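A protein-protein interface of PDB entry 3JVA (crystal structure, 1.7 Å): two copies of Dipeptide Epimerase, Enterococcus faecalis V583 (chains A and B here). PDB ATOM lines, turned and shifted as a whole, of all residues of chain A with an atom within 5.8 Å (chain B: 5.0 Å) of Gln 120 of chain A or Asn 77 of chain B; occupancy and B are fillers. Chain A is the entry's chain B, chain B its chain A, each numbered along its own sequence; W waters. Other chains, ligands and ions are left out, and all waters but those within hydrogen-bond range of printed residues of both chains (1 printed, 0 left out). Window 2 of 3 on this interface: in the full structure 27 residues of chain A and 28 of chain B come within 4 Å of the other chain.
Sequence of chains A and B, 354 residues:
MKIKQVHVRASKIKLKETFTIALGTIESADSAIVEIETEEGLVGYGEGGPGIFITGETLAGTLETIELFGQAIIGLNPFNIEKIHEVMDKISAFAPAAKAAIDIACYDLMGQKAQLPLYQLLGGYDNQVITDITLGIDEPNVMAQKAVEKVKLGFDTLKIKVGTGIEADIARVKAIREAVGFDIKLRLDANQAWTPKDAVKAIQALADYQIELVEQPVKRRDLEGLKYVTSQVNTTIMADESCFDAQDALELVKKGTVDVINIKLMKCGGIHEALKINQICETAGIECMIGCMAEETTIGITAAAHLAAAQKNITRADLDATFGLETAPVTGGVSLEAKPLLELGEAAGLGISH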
ATOM      1  N   LEU A 116     -15.303 -21.799 -15.627  1.00  0.00           N
ATOM      2  CA  LEU A 116     -16.308 -20.744 -15.633  1.00  0.00           C
ATOM      3  C   LEU A 116     -15.681 -19.421 -15.225  1.00  0.00           C
ATOM      4  O   LEU A 116     -14.747 -19.391 -14.417  1.00  0.00           O
ATOM      5  CB  LEU A 116     -17.417 -21.061 -14.626  1.00  0.00           C
ATOM      6  CG  LEU A 116     -18.316 -22.278 -14.835  1.00  0.00           C
ATOM      7  CD1 LEU A 116     -19.118 -22.535 -13.576  1.00  0.00           C
ATOM      8  CD2 LEU A 116     -19.230 -22.035 -16.014  1.00  0.00           C
ATOM      9  N   PRO A 117     -16.172 -18.310 -15.797  1.00  0.00           N
ATOM     10  CA  PRO A 117     -15.630 -17.000 -15.431  1.00  0.00           C
ATOM     11  C   PRO A 117     -16.027 -16.846 -13.966  1.00  0.00           C
ATOM     12  O   PRO A 117     -17.076 -17.344 -13.557  1.00  0.00           O
ATOM     13  CB  PRO A 117     -16.405 -16.036 -16.328  1.00  0.00           C
ATOM     14  CG  PRO A 117     -16.743 -16.870 -17.521  1.00  0.00           C
ATOM     15  CD  PRO A 117     -17.135 -18.189 -16.903  1.00  0.00           C
ATOM     16  N   LEU A 118     -15.218 -16.149 -13.184  1.00  0.00           N
ATOM     17  CA  LEU A 118     -15.511 -16.000 -11.767  1.00  0.00           C
ATOM     18  C   LEU A 118     -16.884 -15.431 -11.424  1.00  0.00           C
ATOM     19  O   LEU A 118     -17.529 -15.901 -10.487  1.00  0.00           O
ATOM     20  CB  LEU A 118     -14.423 -15.157 -11.090  1.00  0.00           C
ATOM     21  CG  LEU A 118     -14.549 -14.963  -9.573  1.00  0.00           C
ATOM     22  CD1 LEU A 118     -14.663 -16.319  -8.861  1.00  0.00           C
ATOM     23  CD2 LEU A 118     -13.331 -14.199  -9.076  1.00  0.00           C
ATOM     24  N   TYR A 119     -17.345 -14.428 -12.166  1.00  0.00           N
ATOM     25  CA  TYR A 119     -18.644 -13.838 -11.855  1.00  0.00           C
ATOM     26  C   TYR A 119     -19.788 -14.848 -11.853  1.00  0.00           C
ATOM     27  O   TYR A 119     -20.810 -14.625 -11.210  1.00  0.00           O
ATOM     28  CB  TYR A 119     -18.956 -12.674 -12.807  1.00  0.00           C
ATOM     29  CG  TYR A 119     -19.207 -13.063 -14.246  1.00  0.00           C
ATOM     30  CD1 TYR A 119     -20.426 -13.610 -14.638  1.00  0.00           C
ATOM     31  CD2 TYR A 119     -18.225 -12.879 -15.214  1.00  0.00           C
ATOM     32  CE1 TYR A 119     -20.663 -13.963 -15.968  1.00  0.00           C
ATOM     33  CE2 TYR A 119     -18.450 -13.230 -16.544  1.00  0.00           C
ATOM     34  CZ  TYR A 119     -19.671 -13.771 -16.912  1.00  0.00           C
ATOM     35  OH  TYR A 119     -19.899 -14.121 -18.225  1.00  0.00           O
ATOM     36  N   GLN A 120     -19.618 -15.963 -12.558  1.00  0.00           N
ATOM     37  CA  GLN A 120     -20.660 -16.983 -12.604  1.00  0.00           C
ATOM     38  C   GLN A 120     -20.717 -17.764 -11.296  1.00  0.00           C
ATOM     39  O   GLN A 120     -21.749 -18.334 -10.949  1.00  0.00           O
ATOM     40  CB  GLN A 120     -20.424 -17.943 -13.777  1.00  0.00           C
ATOM     41  CG  GLN A 120     -20.554 -17.273 -15.142  1.00  0.00           C
ATOM     42  CD  GLN A 120     -21.987 -16.900 -15.487  1.00  0.00           C
ATOM     43  OE1 GLN A 120     -22.800 -16.618 -14.607  1.00  0.00           O
ATOM     44  NE2 GLN A 120     -22.296 -16.883 -16.779  1.00  0.00           N
ATOM     45  N   LEU A 121     -19.606 -17.787 -10.566  1.00  0.00           N
ATOM     46  CA  LEU A 121     -19.567 -18.495  -9.288  1.00  0.00           C
ATOM     47  C   LEU A 121     -19.948 -17.585  -8.129  1.00  0.00           C
ATOM     48  O   LEU A 121     -20.142 -18.056  -7.009  1.00  0.00           O
ATOM     49  CB  LEU A 121     -18.164 -19.048  -9.020  1.00  0.00           C
ATOM     50  CG  LEU A 121     -17.623 -20.145  -9.935  1.00  0.00           C
ATOM     51  CD1 LEU A 121     -16.211 -20.512  -9.502  1.00  0.00           C
ATOM     52  CD2 LEU A 121     -18.538 -21.355  -9.875  1.00  0.00           C
ATOM     53  N   LEU A 122     -20.061 -16.285  -8.393  1.00  0.00           N
ATOM     54  CA  LEU A 122     -20.367 -15.323  -7.342  1.00  0.00           C
ATOM     55  C   LEU A 122     -21.756 -14.684  -7.364  1.00  0.00           C
ATOM     56  O   LEU A 122     -21.988 -13.707  -6.652  1.00  0.00           O
ATOM     57  CB  LEU A 122     -19.304 -14.212  -7.351  1.00  0.00           C
ATOM     58  CG  LEU A 122     -17.845 -14.678  -7.241  1.00  0.00           C
ATOM     59  CD1 LEU A 122     -16.904 -13.481  -7.344  1.00  0.00           C
ATOM     60  CD2 LEU A 122     -17.634 -15.408  -5.912  1.00  0.00           C
ATOM     61  N   GLY A 123     -22.675 -15.215  -8.168  1.00  0.00           N
ATOM     62  CA  GLY A 123     -24.011 -14.638  -8.220  1.00  0.00           C
ATOM     63  C   GLY A 123     -24.577 -14.543  -9.627  1.00  0.00           C
ATOM     64  O   GLY A 123     -25.794 -14.595  -9.816  1.00  0.00           O
ATOM     65  N   GLY A 124     -23.689 -14.381 -10.602  1.00  0.00           N
ATOM     66  CA  GLY A 124     -24.074 -14.308 -12.008  1.00  0.00           C
ATOM     67  C   GLY A 124     -25.058 -13.243 -12.466  1.00  0.00           C
ATOM     68  O   GLY A 124     -25.608 -13.349 -13.562  1.00  0.00           O
ATOM     69  N   HIS A 306     -15.415  -8.831 -10.960  1.00  0.00           N
ATOM     70  CA  HIS A 306     -16.221 -10.044 -11.087  1.00  0.00           C
ATOM     71  C   HIS A 306     -17.256 -10.082  -9.966  1.00  0.00           C
ATOM     72  O   HIS A 306     -18.411 -10.427 -10.188  1.00  0.00           O
ATOM     73  CB  HIS A 306     -15.325 -11.289 -11.028  1.00  0.00           C
ATOM     74  CG  HIS A 306     -14.684 -11.627 -12.340  1.00  0.00           C
ATOM     75  ND1 HIS A 306     -15.228 -12.538 -13.219  1.00  0.00           N
ATOM     76  CD2 HIS A 306     -13.578 -11.133 -12.946  1.00  0.00           C
ATOM     77  CE1 HIS A 306     -14.485 -12.590 -14.310  1.00  0.00           C
ATOM     78  NE2 HIS A 306     -13.478 -11.747 -14.171  1.00  0.00           N
ATOM     79  N   ALA A 310     -21.273  -9.727 -10.429  1.00  0.00           N
ATOM     80  CA  ALA A 310     -22.062 -10.869  -9.974  1.00  0.00           C
ATOM     81  C   ALA A 310     -23.158 -10.588  -8.954  1.00  0.00           C
ATOM     82  O   ALA A 310     -24.183 -11.269  -8.950  1.00  0.00           O
ATOM     83  CB  ALA A 310     -21.132 -11.946  -9.425  1.00  0.00           C
ATOM     84  N   GLU A 346     -15.541 -14.446 -21.225  1.00  0.00           N
ATOM     85  CA  GLU A 346     -15.801 -15.830 -20.852  1.00  0.00           C
ATOM     86  C   GLU A 346     -14.601 -16.659 -20.403  1.00  0.00           C
ATOM     87  O   GLU A 346     -14.737 -17.860 -20.185  1.00  0.00           O
ATOM     88  CB  GLU A 346     -16.506 -16.548 -22.007  1.00  0.00           C
ATOM     89  CG  GLU A 346     -17.935 -16.089 -22.219  1.00  0.00           C
ATOM     90  CD  GLU A 346     -18.816 -16.382 -21.019  1.00  0.00           C
ATOM     91  OE1 GLU A 346     -19.038 -17.575 -20.723  1.00  0.00           O
ATOM     92  OE2 GLU A 346     -19.278 -15.419 -20.367  1.00  0.00           O
ATOM     93  N   MET B   1     -24.941 -21.204 -20.291  1.00  0.00           N
ATOM     94  CA  MET B   1     -26.055 -22.145 -19.987  1.00  0.00           C
ATOM     95  C   MET B   1     -27.365 -21.368 -19.917  1.00  0.00           C
ATOM     96  O   MET B   1     -27.414 -20.266 -19.364  1.00  0.00           O
ATOM     97  CB  MET B   1     -25.775 -22.867 -18.661  1.00  0.00           C
ATOM     98  CG  MET B   1     -26.809 -23.912 -18.265  1.00  0.00           C
ATOM     99  SD  MET B   1     -26.165 -25.123 -17.058  1.00  0.00           S
ATOM    100  CE  MET B   1     -25.861 -24.079 -15.670  1.00  0.00           C
ATOM    101  N   LYS B   2     -28.424 -21.931 -20.490  1.00  0.00           N
ATOM    102  CA  LYS B   2     -29.722 -21.267 -20.495  1.00  0.00           C
ATOM    103  C   LYS B   2     -30.872 -22.219 -20.210  1.00  0.00           C
ATOM    104  O   LYS B   2     -30.891 -23.352 -20.688  1.00  0.00           O
ATOM    105  CB  LYS B   2     -29.953 -20.578 -21.846  1.00  0.00           C
ATOM    106  CG  LYS B   2     -28.956 -19.467 -22.151  1.00  0.00           C
ATOM    107  CD  LYS B   2     -29.148 -18.901 -23.557  1.00  0.00           C
ATOM    108  CE  LYS B   2     -30.543 -18.328 -23.751  1.00  0.00           C
ATOM    109  NZ  LYS B   2     -30.714 -17.747 -25.117  1.00  0.00           N
ATOM    110  N   ILE B   3     -31.830 -21.752 -19.416  1.00  0.00           N
ATOM    111  CA  ILE B   3     -32.994 -22.555 -19.065  1.00  0.00           C
ATOM    112  C   ILE B   3     -33.914 -22.688 -20.277  1.00  0.00           C
ATOM    113  O   ILE B   3     -34.352 -21.692 -20.848  1.00  0.00           O
ATOM    114  CB  ILE B   3     -33.774 -21.911 -17.895  1.00  0.00           C
ATOM    115  CG1 ILE B   3     -32.900 -21.912 -16.634  1.00  0.00           C
ATOM    116  CG2 ILE B   3     -35.082 -22.665 -17.645  1.00  0.00           C
ATOM    117  CD1 ILE B   3     -33.546 -21.252 -15.427  1.00  0.00           C
ATOM    118  N   GLY B  75     -34.987 -18.955 -20.403  1.00  0.00           N
ATOM    119  CA  GLY B  75     -33.968 -18.135 -21.039  1.00  0.00           C
ATOM    120  C   GLY B  75     -32.884 -17.604 -20.113  1.00  0.00           C
ATOM    121  O   GLY B  75     -31.870 -17.088 -20.583  1.00  0.00           O
ATOM    122  N   LEU B  76     -33.084 -17.725 -18.805  1.00  0.00           N
ATOM    123  CA  LEU B  76     -32.085 -17.247 -17.849  1.00  0.00           C
ATOM    124  C   LEU B  76     -30.989 -18.282 -17.594  1.00  0.00           C
ATOM    125  O   LEU B  76     -31.177 -19.478 -17.812  1.00  0.00           O
ATOM    126  CB  LEU B  76     -32.747 -16.876 -16.514  1.00  0.00           C
ATOM    127  CG  LEU B  76     -33.735 -15.706 -16.486  1.00  0.00           C
ATOM    128  CD1 LEU B  76     -34.188 -15.456 -15.048  1.00  0.00           C
ATOM    129  CD2 LEU B  76     -33.077 -14.451 -17.057  1.00  0.00           C
ATOM    130  N   ASN B  77     -29.836 -17.806 -17.139  1.00  0.00           N
ATOM    131  CA  ASN B  77     -28.715 -18.681 -16.832  1.00  0.00           C
ATOM    132  C   ASN B  77     -28.896 -19.166 -15.389  1.00  0.00           C
ATOM    133  O   ASN B  77     -29.081 -18.354 -14.486  1.00  0.00           O
ATOM    134  CB  ASN B  77     -27.405 -17.902 -16.941  1.00  0.00           C
ATOM    135  CG  ASN B  77     -26.188 -18.803 -16.917  1.00  0.00           C
ATOM    136  OD1 ASN B  77     -26.130 -19.769 -16.157  1.00  0.00           O
ATOM    137  ND2 ASN B  77     -25.203 -18.484 -17.748  1.00  0.00           N
ATOM    138  N   PRO B  78     -28.860 -20.493 -15.159  1.00  0.00           N
ATOM    139  CA  PRO B  78     -29.021 -21.042 -13.808  1.00  0.00           C
ATOM    140  C   PRO B  78     -28.013 -20.459 -12.819  1.00  0.00           C
ATOM    141  O   PRO B  78     -28.270 -20.425 -11.612  1.00  0.00           O
ATOM    142  CB  PRO B  78     -28.817 -22.542 -14.016  1.00  0.00           C
ATOM    143  CG  PRO B  78     -29.379 -22.759 -15.385  1.00  0.00           C
ATOM    144  CD  PRO B  78     -28.820 -21.575 -16.161  1.00  0.00           C
ATOM    145  N   PHE B  79     -26.867 -20.025 -13.334  1.00  0.00           N
ATOM    146  CA  PHE B  79     -25.824 -19.427 -12.501  1.00  0.00           C
ATOM    147  C   PHE B  79     -26.229 -18.044 -12.020  1.00  0.00           C
ATOM    148  O   PHE B  79     -25.674 -17.532 -11.047  1.00  0.00           O
ATOM    149  CB  PHE B  79     -24.509 -19.329 -13.275  1.00  0.00           C
ATOM    150  CG  PHE B  79     -23.734 -20.607 -13.302  1.00  0.00           C
ATOM    151  CD1 PHE B  79     -23.082 -21.059 -12.161  1.00  0.00           C
ATOM    152  CD2 PHE B  79     -23.681 -21.379 -14.457  1.00  0.00           C
ATOM    153  CE1 PHE B  79     -22.382 -22.272 -12.167  1.00  0.00           C
ATOM    154  CE2 PHE B  79     -22.989 -22.588 -14.473  1.00  0.00           C
ATOM    155  CZ  PHE B  79     -22.340 -23.033 -13.326  1.00  0.00           C
ATOM    156  N   ASN B  80     -27.183 -17.433 -12.712  1.00  0.00           N
ATOM    157  CA  ASN B  80     -27.658 -16.107 -12.329  1.00  0.00           C
ATOM    158  C   ASN B  80     -28.691 -16.292 -11.222  1.00  0.00           C
ATOM    159  O   ASN B  80     -29.873 -15.971 -11.381  1.00  0.00           O
ATOM    160  CB  ASN B  80     -28.293 -15.403 -13.527  1.00  0.00           C
ATOM    161  CG  ASN B  80     -28.502 -13.922 -13.279  1.00  0.00           C
ATOM    162  OD1 ASN B  80     -28.400 -13.449 -12.143  1.00  0.00           O
ATOM    163  ND2 ASN B  80     -28.800 -13.180 -14.341  1.00  0.00           N
ATOM    164  N   ILE B  81     -28.230 -16.825 -10.092  1.00  0.00           N
ATOM    165  CA  ILE B  81     -29.101 -17.092  -8.962  1.00  0.00           C
ATOM    166  C   ILE B  81     -29.623 -15.781  -8.367  1.00  0.00           C
ATOM    167  O   ILE B  81     -30.688 -15.742  -7.743  1.00  0.00           O
ATOM    168  CB  ILE B  81     -28.344 -17.954  -7.905  1.00  0.00           C
ATOM    169  CG1 ILE B  81     -29.322 -18.470  -6.846  1.00  0.00           C
ATOM    170  CG2 ILE B  81     -27.188 -17.160  -7.296  1.00  0.00           C
ATOM    171  CD1 ILE B  81     -30.436 -19.345  -7.425  1.00  0.00           C
ATOM    172  N   ILE B  84     -32.596 -14.845 -10.655  1.00  0.00           N
ATOM    173  CA  ILE B  84     -33.649 -15.827 -10.478  1.00  0.00           C
ATOM    174  C   ILE B  84     -34.441 -15.525  -9.210  1.00  0.00           C
ATOM    175  O   ILE B  84     -35.664 -15.563  -9.214  1.00  0.00           O
ATOM    176  CB  ILE B  84     -33.057 -17.259 -10.455  1.00  0.00           C
ATOM    177  CG1 ILE B  84     -32.590 -17.620 -11.871  1.00  0.00           C
ATOM    178  CG2 ILE B  84     -34.096 -18.267  -9.972  1.00  0.00           C
ATOM    179  CD1 ILE B  84     -31.782 -18.891 -11.963  1.00  0.00           C
HETATM  180  O   HOH W   1     -23.646 -17.825  -9.160  1.00  0.00           O
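Hydrophobic or aromatic side chains of chain A within 4 Å of the printed part of chain B: Leu 116. Printed residues of chain B that touch a printed residue of chain A: Asn 77, Phe 79, Asn 80 and Ile 81. Hydrophobic or aromatic side chains of chain B within 4 Å of the printed part of chain A: Phe 79 and Ile 81. Among the printed residues, 8 pairs touch across the chains.
N of Ile 81 of chain B sits at hydrogen-bond distance from O of Gly 123 of chain A (3.3 Å). The side-chain amide nitrogen of Asn 77 of chain B lies close to the side-chain amide nitrogen of Gln 120 of chain A. The side-chain amide oxygen of Asn 80 of chain B lies close to the backbone carbonyl oxygen of Gly 124 of chain A. The backbone carbonyl oxygen (O) of Gly 123 of chain A sits close to the backbone carbonyl oxygen (O) of Phe 79 of chain B (3.2 Å).
Water W1 lies within hydrogen-bond range of O of Gln 120 of chain A (2.7 Å), O of Phe 79 of chain B (2.8 Å) and N of Gly 123 of chain A (3.0 Å).
The backbone carbonyl oxygen (O) of Tyr 119 of chain A is in hydrogen-bond range of the backbone NH (N) of Gly 124 of chain A, 3.0 Å away. The side-chain amide oxygen (OD1) of Asn 77 of chain B lies within hydrogen-bond range of the backbone NH (N) of Phe 79 of chain B, 2.9 Å away. O of Met 1 of chain B sits close to ND2 of Asn 77 of chain B, 3.3 Å away.
Among the printed residues, merely in contact across the chains: Gln 120 of chain A with Phe 79 of chain B, Leu 116 of chain A with Phe 79 of chain B, Gly 123 of chain A with Asn 80 of chain B and Gly 124 of chain A with Phe 79 of chain B.
Of the printed residues of chain B, Leu 116 of chain A touches Phe 79 (3.3 Å). Gln 120 of chain A touches just these residues of chain B: Asn 77 and Phe 79. Printed residues of chain B within 4 Å of Gly 124 of chain A: Phe 79 (3.7 Å) and Asn 80 (3.0 Å). Lys 2 of chain B touches none of the printed residues of chain A. Asn 77 of chain B touches just one residue of chain A: Gln 120. Pro 78 of chain B touches none of the printed residues of chain A. Printed residues of chain A within 4 Å of Asn 80 of chain B: Gly 123 (3.5 Å) and Gly 124 (3.0 Å). Of the printed residues of chain A, Ile 81 of chain B touches Gly 123 (3.3 Å). The nearest printed residue of chain B that does not touch Gly 123 of chain A is Pro 78 of chain B (6.6 Å).
No position is printed for both chains.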
